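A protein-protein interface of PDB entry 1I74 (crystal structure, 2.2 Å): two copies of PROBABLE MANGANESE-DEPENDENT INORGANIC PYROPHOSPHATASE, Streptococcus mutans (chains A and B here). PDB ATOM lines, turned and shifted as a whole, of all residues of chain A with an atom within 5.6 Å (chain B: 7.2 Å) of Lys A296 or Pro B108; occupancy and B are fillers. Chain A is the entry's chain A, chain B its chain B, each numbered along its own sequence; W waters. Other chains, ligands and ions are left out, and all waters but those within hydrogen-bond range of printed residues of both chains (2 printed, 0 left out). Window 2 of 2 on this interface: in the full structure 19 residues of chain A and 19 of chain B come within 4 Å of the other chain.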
ATOM      1  N   HIS A  97     -22.006 -29.915  31.889  1.00  0.00           N
ATOM      2  CA  HIS A  97     -22.002 -29.094  30.691  1.00  0.00           C
ATOM      3  C   HIS A  97     -22.703 -27.755  30.896  1.00  0.00           C
ATOM      4  O   HIS A  97     -23.226 -27.164  29.953  1.00  0.00           O
ATOM      5  CB  HIS A  97     -22.628 -29.838  29.502  1.00  0.00           C
ATOM      6  CG  HIS A  97     -24.061 -30.227  29.698  1.00  0.00           C
ATOM      7  ND1 HIS A  97     -25.024 -30.006  28.739  1.00  0.00           N
ATOM      8  CD2 HIS A  97     -24.687 -30.857  30.721  1.00  0.00           C
ATOM      9  CE1 HIS A  97     -26.181 -30.482  29.163  1.00  0.00           C
ATOM     10  NE2 HIS A  97     -26.004 -31.004  30.362  1.00  0.00           N
ATOM     11  N   HIS A  98     -22.706 -27.276  32.133  1.00  0.00           N
ATOM     12  CA  HIS A  98     -23.325 -26.001  32.440  1.00  0.00           C
ATOM     13  C   HIS A  98     -22.282 -24.974  32.826  1.00  0.00           C
ATOM     14  O   HIS A  98     -21.116 -25.303  33.077  1.00  0.00           O
ATOM     15  CB  HIS A  98     -24.302 -26.125  33.603  1.00  0.00           C
ATOM     16  CG  HIS A  98     -25.457 -27.030  33.332  1.00  0.00           C
ATOM     17  ND1 HIS A  98     -25.398 -28.392  33.532  1.00  0.00           N
ATOM     18  CD2 HIS A  98     -26.704 -26.768  32.880  1.00  0.00           C
ATOM     19  CE1 HIS A  98     -26.560 -28.930  33.219  1.00  0.00           C
ATOM     20  NE2 HIS A  98     -27.371 -27.966  32.820  1.00  0.00           N
ATOM     21  N   ARG A  99     -22.713 -23.722  32.883  1.00  0.00           N
ATOM     22  CA  ARG A  99     -21.823 -22.669  33.297  1.00  0.00           C
ATOM     23  C   ARG A  99     -21.487 -22.981  34.764  1.00  0.00           C
ATOM     24  O   ARG A  99     -22.166 -23.771  35.413  1.00  0.00           O
ATOM     25  CB  ARG A  99     -22.508 -21.302  33.142  1.00  0.00           C
ATOM     26  CG  ARG A  99     -23.785 -21.065  33.970  1.00  0.00           C
ATOM     27  CD  ARG A  99     -23.481 -20.783  35.439  1.00  0.00           C
ATOM     28  NE  ARG A  99     -24.604 -20.145  36.137  1.00  0.00           N
ATOM     29  CZ  ARG A  99     -24.761 -18.829  36.255  1.00  0.00           C
ATOM     30  NH1 ARG A  99     -23.864 -18.005  35.724  1.00  0.00           N
ATOM     31  NH2 ARG A  99     -25.805 -18.331  36.912  1.00  0.00           N
ATOM     32  N   GLU A 114     -17.581 -29.561  29.479  1.00  0.00           N
ATOM     33  CA  GLU A 114     -17.502 -29.311  28.046  1.00  0.00           C
ATOM     34  C   GLU A 114     -18.801 -28.630  27.642  1.00  0.00           C
ATOM     35  O   GLU A 114     -19.875 -29.012  28.087  1.00  0.00           O
ATOM     36  CB  GLU A 114     -17.327 -30.624  27.266  1.00  0.00           C
ATOM     37  CG  GLU A 114     -16.266 -31.554  27.824  1.00  0.00           C
ATOM     38  CD  GLU A 114     -15.913 -32.688  26.873  1.00  0.00           C
ATOM     39  OE1 GLU A 114     -16.783 -33.091  26.079  1.00  0.00           O
ATOM     40  OE2 GLU A 114     -14.765 -33.182  26.922  1.00  0.00           O
ATOM     41  N   PRO A 115     -18.717 -27.593  26.801  1.00  0.00           N
ATOM     42  CA  PRO A 115     -19.941 -26.904  26.385  1.00  0.00           C
ATOM     43  C   PRO A 115     -20.713 -27.702  25.329  1.00  0.00           C
ATOM     44  O   PRO A 115     -20.939 -27.222  24.225  1.00  0.00           O
ATOM     45  CB  PRO A 115     -19.410 -25.577  25.855  1.00  0.00           C
ATOM     46  CG  PRO A 115     -18.120 -26.004  25.202  1.00  0.00           C
ATOM     47  CD  PRO A 115     -17.522 -26.951  26.224  1.00  0.00           C
ATOM     48  N   THR A 157     -29.255 -26.705  21.623  1.00  0.00           N
ATOM     49  CA  THR A 157     -28.177 -27.055  22.544  1.00  0.00           C
ATOM     50  C   THR A 157     -27.331 -28.160  21.949  1.00  0.00           C
ATOM     51  O   THR A 157     -26.242 -28.448  22.436  1.00  0.00           O
ATOM     52  CB  THR A 157     -28.702 -27.543  23.900  1.00  0.00           C
ATOM     53  OG1 THR A 157     -29.530 -28.701  23.708  1.00  0.00           O
ATOM     54  CG2 THR A 157     -29.487 -26.436  24.588  1.00  0.00           C
ATOM     55  N   LYS A 205     -35.926 -25.300  37.930  1.00  0.00           N
ATOM     56  CA  LYS A 205     -34.763 -24.729  38.603  1.00  0.00           C
ATOM     57  C   LYS A 205     -35.064 -23.287  38.968  1.00  0.00           C
ATOM     58  O   LYS A 205     -35.991 -22.682  38.431  1.00  0.00           O
ATOM     59  CB  LYS A 205     -33.533 -24.754  37.690  1.00  0.00           C
ATOM     60  CG  LYS A 205     -33.167 -26.123  37.194  1.00  0.00           C
ATOM     61  CD  LYS A 205     -31.858 -26.127  36.386  1.00  0.00           C
ATOM     62  CE  LYS A 205     -32.011 -25.450  35.028  1.00  0.00           C
ATOM     63  NZ  LYS A 205     -30.913 -25.837  34.084  1.00  0.00           N
ATOM     64  N   SER A 294     -35.770 -25.054  24.190  1.00  0.00           N
ATOM     65  CA  SER A 294     -34.705 -25.062  25.182  1.00  0.00           C
ATOM     66  C   SER A 294     -34.863 -23.953  26.210  1.00  0.00           C
ATOM     67  O   SER A 294     -34.924 -22.774  25.862  1.00  0.00           O
ATOM     68  CB  SER A 294     -33.339 -24.917  24.503  1.00  0.00           C
ATOM     69  OG  SER A 294     -32.349 -24.480  25.422  1.00  0.00           O
ATOM     70  N   ARG A 295     -34.922 -24.337  27.480  1.00  0.00           N
ATOM     71  CA  ARG A 295     -35.048 -23.362  28.543  1.00  0.00           C
ATOM     72  C   ARG A 295     -33.767 -22.537  28.629  1.00  0.00           C
ATOM     73  O   ARG A 295     -33.816 -21.312  28.574  1.00  0.00           O
ATOM     74  CB  ARG A 295     -35.330 -24.052  29.889  1.00  0.00           C
ATOM     75  CG  ARG A 295     -35.288 -23.117  31.106  1.00  0.00           C
ATOM     76  CD  ARG A 295     -35.740 -23.819  32.385  1.00  0.00           C
ATOM     77  NE  ARG A 295     -35.022 -25.073  32.618  1.00  0.00           N
ATOM     78  CZ  ARG A 295     -35.489 -26.082  33.354  1.00  0.00           C
ATOM     79  NH1 ARG A 295     -36.677 -25.992  33.943  1.00  0.00           N
ATOM     80  NH2 ARG A 295     -34.777 -27.194  33.483  1.00  0.00           N
ATOM     81  N   LYS A 296     -32.619 -23.208  28.727  1.00  0.00           N
ATOM     82  CA  LYS A 296     -31.345 -22.494  28.858  1.00  0.00           C
ATOM     83  C   LYS A 296     -30.978 -21.559  27.712  1.00  0.00           C
ATOM     84  O   LYS A 296     -30.345 -20.529  27.939  1.00  0.00           O
ATOM     85  CB  LYS A 296     -30.194 -23.476  29.090  1.00  0.00           C
ATOM     86  CG  LYS A 296     -29.777 -24.292  27.868  1.00  0.00           C
ATOM     87  CD  LYS A 296     -28.655 -25.279  28.214  1.00  0.00           C
ATOM     88  CE  LYS A 296     -27.387 -24.579  28.737  1.00  0.00           C
ATOM     89  NZ  LYS A 296     -26.400 -25.571  29.318  1.00  0.00           N
ATOM     90  N   LYS A 297     -31.385 -21.896  26.492  1.00  0.00           N
ATOM     91  CA  LYS A 297     -31.056 -21.057  25.341  1.00  0.00           C
ATOM     92  C   LYS A 297     -32.159 -20.110  24.863  1.00  0.00           C
ATOM     93  O   LYS A 297     -31.880 -18.994  24.425  1.00  0.00           O
ATOM     94  CB  LYS A 297     -30.630 -21.929  24.151  1.00  0.00           C
ATOM     95  CG  LYS A 297     -29.164 -22.364  24.126  1.00  0.00           C
ATOM     96  CD  LYS A 297     -28.668 -22.401  22.673  1.00  0.00           C
ATOM     97  CE  LYS A 297     -27.204 -22.805  22.536  1.00  0.00           C
ATOM     98  NZ  LYS A 297     -26.268 -21.920  23.276  1.00  0.00           N
ATOM     99  N   GLN A 298     -33.411 -20.544  24.953  1.00  0.00           N
ATOM    100  CA  GLN A 298     -34.504 -19.731  24.458  1.00  0.00           C
ATOM    101  C   GLN A 298     -35.427 -19.066  25.464  1.00  0.00           C
ATOM    102  O   GLN A 298     -36.380 -18.403  25.074  1.00  0.00           O
ATOM    103  CB  GLN A 298     -35.323 -20.563  23.475  1.00  0.00           C
ATOM    104  CG  GLN A 298     -34.543 -20.932  22.220  1.00  0.00           C
ATOM    105  CD  GLN A 298     -35.213 -22.026  21.418  1.00  0.00           C
ATOM    106  OE1 GLN A 298     -35.332 -23.165  21.878  1.00  0.00           O
ATOM    107  NE2 GLN A 298     -35.664 -21.688  20.219  1.00  0.00           N
ATOM    108  N   VAL A 299     -35.149 -19.214  26.751  1.00  0.00           N
ATOM    109  CA  VAL A 299     -35.999 -18.594  27.756  1.00  0.00           C
ATOM    110  C   VAL A 299     -35.222 -17.818  28.811  1.00  0.00           C
ATOM    111  O   VAL A 299     -35.397 -16.606  28.946  1.00  0.00           O
ATOM    112  CB  VAL A 299     -36.884 -19.644  28.440  1.00  0.00           C
ATOM    113  CG1 VAL A 299     -37.588 -19.037  29.642  1.00  0.00           C
ATOM    114  CG2 VAL A 299     -37.904 -20.168  27.445  1.00  0.00           C
ATOM    115  N   VAL A 300     -34.363 -18.507  29.557  1.00  0.00           N
ATOM    116  CA  VAL A 300     -33.579 -17.850  30.589  1.00  0.00           C
ATOM    117  C   VAL A 300     -32.814 -16.616  30.088  1.00  0.00           C
ATOM    118  O   VAL A 300     -32.846 -15.559  30.720  1.00  0.00           O
ATOM    119  CB  VAL A 300     -32.583 -18.834  31.235  1.00  0.00           C
ATOM    120  CG1 VAL A 300     -31.668 -18.091  32.196  1.00  0.00           C
ATOM    121  CG2 VAL A 300     -33.345 -19.927  31.973  1.00  0.00           C
ATOM    122  N   PRO A 301     -32.107 -16.738  28.952  1.00  0.00           N
ATOM    123  CA  PRO A 301     -31.346 -15.609  28.402  1.00  0.00           C
ATOM    124  C   PRO A 301     -32.141 -14.314  28.243  1.00  0.00           C
ATOM    125  O   PRO A 301     -31.667 -13.239  28.609  1.00  0.00           O
ATOM    126  CB  PRO A 301     -30.851 -16.154  27.068  1.00  0.00           C
ATOM    127  CG  PRO A 301     -30.593 -17.591  27.397  1.00  0.00           C
ATOM    128  CD  PRO A 301     -31.849 -17.962  28.175  1.00  0.00           C
ATOM    129  N   GLN A 302     -33.345 -14.410  27.699  1.00  0.00           N
ATOM    130  CA  GLN A 302     -34.171 -13.225  27.515  1.00  0.00           C
ATOM    131  C   GLN A 302     -34.729 -12.763  28.850  1.00  0.00           C
ATOM    132  O   GLN A 302     -34.920 -11.565  29.066  1.00  0.00           O
ATOM    133  CB  GLN A 302     -35.308 -13.511  26.538  1.00  0.00           C
ATOM    134  CG  GLN A 302     -35.566 -14.985  26.305  1.00  0.00           C
ATOM    135  CD  GLN A 302     -34.410 -15.696  25.624  1.00  0.00           C
ATOM    136  OE1 GLN A 302     -34.053 -15.378  24.491  1.00  0.00           O
ATOM    137  NE2 GLN A 302     -33.818 -16.663  26.317  1.00  0.00           N
ATOM    138  N   GLU B  90     -14.776 -13.384  28.428  1.00  0.00           N
ATOM    139  CA  GLU B  90     -15.342 -14.713  28.495  1.00  0.00           C
ATOM    140  C   GLU B  90     -14.227 -15.737  28.714  1.00  0.00           C
ATOM    141  O   GLU B  90     -13.200 -15.727  28.027  1.00  0.00           O
ATOM    142  CB  GLU B  90     -16.087 -15.025  27.205  1.00  0.00           C
ATOM    143  CG  GLU B  90     -16.578 -16.443  27.148  1.00  0.00           C
ATOM    144  CD  GLU B  90     -17.392 -16.733  25.911  1.00  0.00           C
ATOM    145  OE1 GLU B  90     -16.919 -16.424  24.788  1.00  0.00           O
ATOM    146  OE2 GLU B  90     -18.506 -17.286  26.064  1.00  0.00           O
ATOM    147  N   VAL B  91     -14.423 -16.602  29.699  1.00  0.00           N
ATOM    148  CA  VAL B  91     -13.452 -17.647  30.008  1.00  0.00           C
ATOM    149  C   VAL B  91     -13.925 -18.857  29.225  1.00  0.00           C
ATOM    150  O   VAL B  91     -14.919 -19.476  29.576  1.00  0.00           O
ATOM    151  CB  VAL B  91     -13.450 -17.971  31.519  1.00  0.00           C
ATOM    152  CG1 VAL B  91     -12.605 -19.203  31.795  1.00  0.00           C
ATOM    153  CG2 VAL B  91     -12.917 -16.783  32.292  1.00  0.00           C
ATOM    154  N   VAL B  92     -13.219 -19.187  28.154  1.00  0.00           N
ATOM    155  CA  VAL B  92     -13.625 -20.301  27.319  1.00  0.00           C
ATOM    156  C   VAL B  92     -13.105 -21.656  27.758  1.00  0.00           C
ATOM    157  O   VAL B  92     -13.705 -22.679  27.444  1.00  0.00           O
ATOM    158  CB  VAL B  92     -13.228 -20.051  25.850  1.00  0.00           C
ATOM    159  CG1 VAL B  92     -14.086 -18.940  25.273  1.00  0.00           C
ATOM    160  CG2 VAL B  92     -11.761 -19.678  25.759  1.00  0.00           C
ATOM    161  N   THR B 105     -18.728 -18.288  35.598  1.00  0.00           N
ATOM    162  CA  THR B 105     -18.905 -18.039  34.176  1.00  0.00           C
ATOM    163  C   THR B 105     -20.384 -17.865  33.884  1.00  0.00           C
ATOM    164  O   THR B 105     -21.235 -18.455  34.544  1.00  0.00           O
ATOM    165  CB  THR B 105     -18.374 -19.206  33.323  1.00  0.00           C
ATOM    166  OG1 THR B 105     -19.258 -20.331  33.442  1.00  0.00           O
ATOM    167  CG2 THR B 105     -16.972 -19.602  33.785  1.00  0.00           C
ATOM    168  N   ALA B 106     -20.685 -17.049  32.889  1.00  0.00           N
ATOM    169  CA  ALA B 106     -22.064 -16.810  32.510  1.00  0.00           C
ATOM    170  C   ALA B 106     -22.557 -17.949  31.624  1.00  0.00           C
ATOM    171  O   ALA B 106     -23.729 -18.312  31.651  1.00  0.00           O
ATOM    172  CB  ALA B 106     -22.174 -15.474  31.761  1.00  0.00           C
ATOM    173  N   ASN B 107     -21.643 -18.529  30.856  1.00  0.00           N
ATOM    174  CA  ASN B 107     -21.991 -19.597  29.928  1.00  0.00           C
ATOM    175  C   ASN B 107     -21.173 -20.866  30.138  1.00  0.00           C
ATOM    176  O   ASN B 107     -20.176 -20.857  30.846  1.00  0.00           O
ATOM    177  CB  ASN B 107     -21.784 -19.090  28.496  1.00  0.00           C
ATOM    178  CG  ASN B 107     -22.690 -17.928  28.160  1.00  0.00           C
ATOM    179  OD1 ASN B 107     -23.880 -18.113  27.908  1.00  0.00           O
ATOM    180  ND2 ASN B 107     -22.141 -16.718  28.175  1.00  0.00           N
ATOM    181  N   PRO B 108     -21.607 -21.983  29.531  1.00  0.00           N
ATOM    182  CA  PRO B 108     -20.889 -23.253  29.659  1.00  0.00           C
ATOM    183  C   PRO B 108     -19.494 -23.076  29.076  1.00  0.00           C
ATOM    184  O   PRO B 108     -19.290 -22.211  28.230  1.00  0.00           O
ATOM    185  CB  PRO B 108     -21.733 -24.210  28.829  1.00  0.00           C
ATOM    186  CG  PRO B 108     -23.121 -23.659  28.984  1.00  0.00           C
ATOM    187  CD  PRO B 108     -22.891 -22.176  28.834  1.00  0.00           C
ATOM    188  N   LEU B 109     -18.539 -23.882  29.531  1.00  0.00           N
ATOM    189  CA  LEU B 109     -17.168 -23.795  29.041  1.00  0.00           C
ATOM    190  C   LEU B 109     -16.456 -25.133  29.165  1.00  0.00           C
ATOM    191  O   LEU B 109     -16.992 -26.085  29.729  1.00  0.00           O
ATOM    192  CB  LEU B 109     -16.376 -22.755  29.839  1.00  0.00           C
ATOM    193  CG  LEU B 109     -16.014 -23.167  31.273  1.00  0.00           C
ATOM    194  CD1 LEU B 109     -15.029 -22.191  31.883  1.00  0.00           C
ATOM    195  CD2 LEU B 109     -17.273 -23.228  32.104  1.00  0.00           C
ATOM    196  N   TYR B 110     -15.241 -25.193  28.634  1.00  0.00           N
ATOM    197  CA  TYR B 110     -14.436 -26.394  28.728  1.00  0.00           C
ATOM    198  C   TYR B 110     -13.552 -26.245  29.959  1.00  0.00           C
ATOM    199  O   TYR B 110     -12.847 -25.252  30.110  1.00  0.00           O
ATOM    200  CB  TYR B 110     -13.543 -26.582  27.494  1.00  0.00           C
ATOM    201  CG  TYR B 110     -12.721 -27.864  27.566  1.00  0.00           C
ATOM    202  CD1 TYR B 110     -13.335 -29.113  27.428  1.00  0.00           C
ATOM    203  CD2 TYR B 110     -11.349 -27.837  27.883  1.00  0.00           C
ATOM    204  CE1 TYR B 110     -12.613 -30.308  27.617  1.00  0.00           C
ATOM    205  CE2 TYR B 110     -10.614 -29.033  28.073  1.00  0.00           C
ATOM    206  CZ  TYR B 110     -11.258 -30.259  27.943  1.00  0.00           C
ATOM    207  OH  TYR B 110     -10.589 -31.446  28.174  1.00  0.00           O
HETATM  208  O   HOH W   1     -19.686 -26.291  30.721  1.00  0.00           O
HETATM  209  O   HOH W   2     -26.231 -17.556  33.563  1.00  0.00           O
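Of the printed residues of chain B, His A97 touches Pro B108 (3.5 Å). Of the printed residues of chain B, His A98 touches Pro B108 (3.9 Å). Of chain B, only Pro B108 (3.8 Å) comes within 4 Å of Lys A296. Of the printed residues of chain A, Ala B106 touches Arg A99 (3.6 Å). Printed residues of chain A within 4 Å of Asn B107: Arg A99 (3.3 Å). The nearest printed residue of chain A that does not touch Pro B108 is Pro A115 (4.01 Å). The nearest printed residue of chain B that does not touch Pro A115 is Pro B108 (4.01 Å).
NH1 of Arg A99 is in hydrogen-bond range of O of Thr B105, at 2.9 Å.
Water W1 bridges the backbone carbonyl oxygen (O) of Leu B109 (2.9 Å) and the backbone carbonyl oxygen (O) of His A98 (2.9 Å). Water W2 lies within hydrogen-bond range of the guanidinium group (NH1) of Arg A99 (3.2 Å) and the backbone carbonyl oxygen (O) of Ala B106 (3.2 Å).
Among the printed residues, pairs that only touch across the chains: Arg A99 with Asn B107 (3.3 Å), His A97 with Pro B108 (3.5 Å), Glu A114 with Leu B109 (3.5 Å), Arg A99 with Ala B106 (3.6 Å), Pro A115 with Leu B109 (3.6 Å), Glu A114 with Tyr B110 (3.7 Å), Arg A99 with Pro B108 (3.7 Å), Pro A115 with Tyr B110 (3.8 Å), Lys A296 with Pro B108 (3.8 Å) and His A98 with Pro B108 (3.9 Å).
The backbone carbonyl oxygen (O) of Val B92 is in hydrogen-bond range of the backbone NH (N) of Tyr B110. The backbone carbonyl oxygen (O) of Asn B107 lies within hydrogen-bond range of the side-chain hydroxyl (OG1) of Thr B105, 2.8 Å away.
No position is printed for both chains. Of the 11 pairs that touch across the chains among the printed residues, none has its exchanged pair printed and touching as well.
Hydrophobic or aromatic side chains of chain B within 4 Å of the printed part of chain A: Pro B108 and Tyr B110. Of the 16 printed residues of chain A, 6 touch a printed residue of chain B. Hydrophobic or aromatic side chains of chain A that line the printed part of chain B: Pro A115. Among the printed residues, 11 pairs touch across the chains. Among the printed residues, no Asp or Glu carboxylate lies within 4 Å of a Lys or Arg side-chain nitrogen of the other chain.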
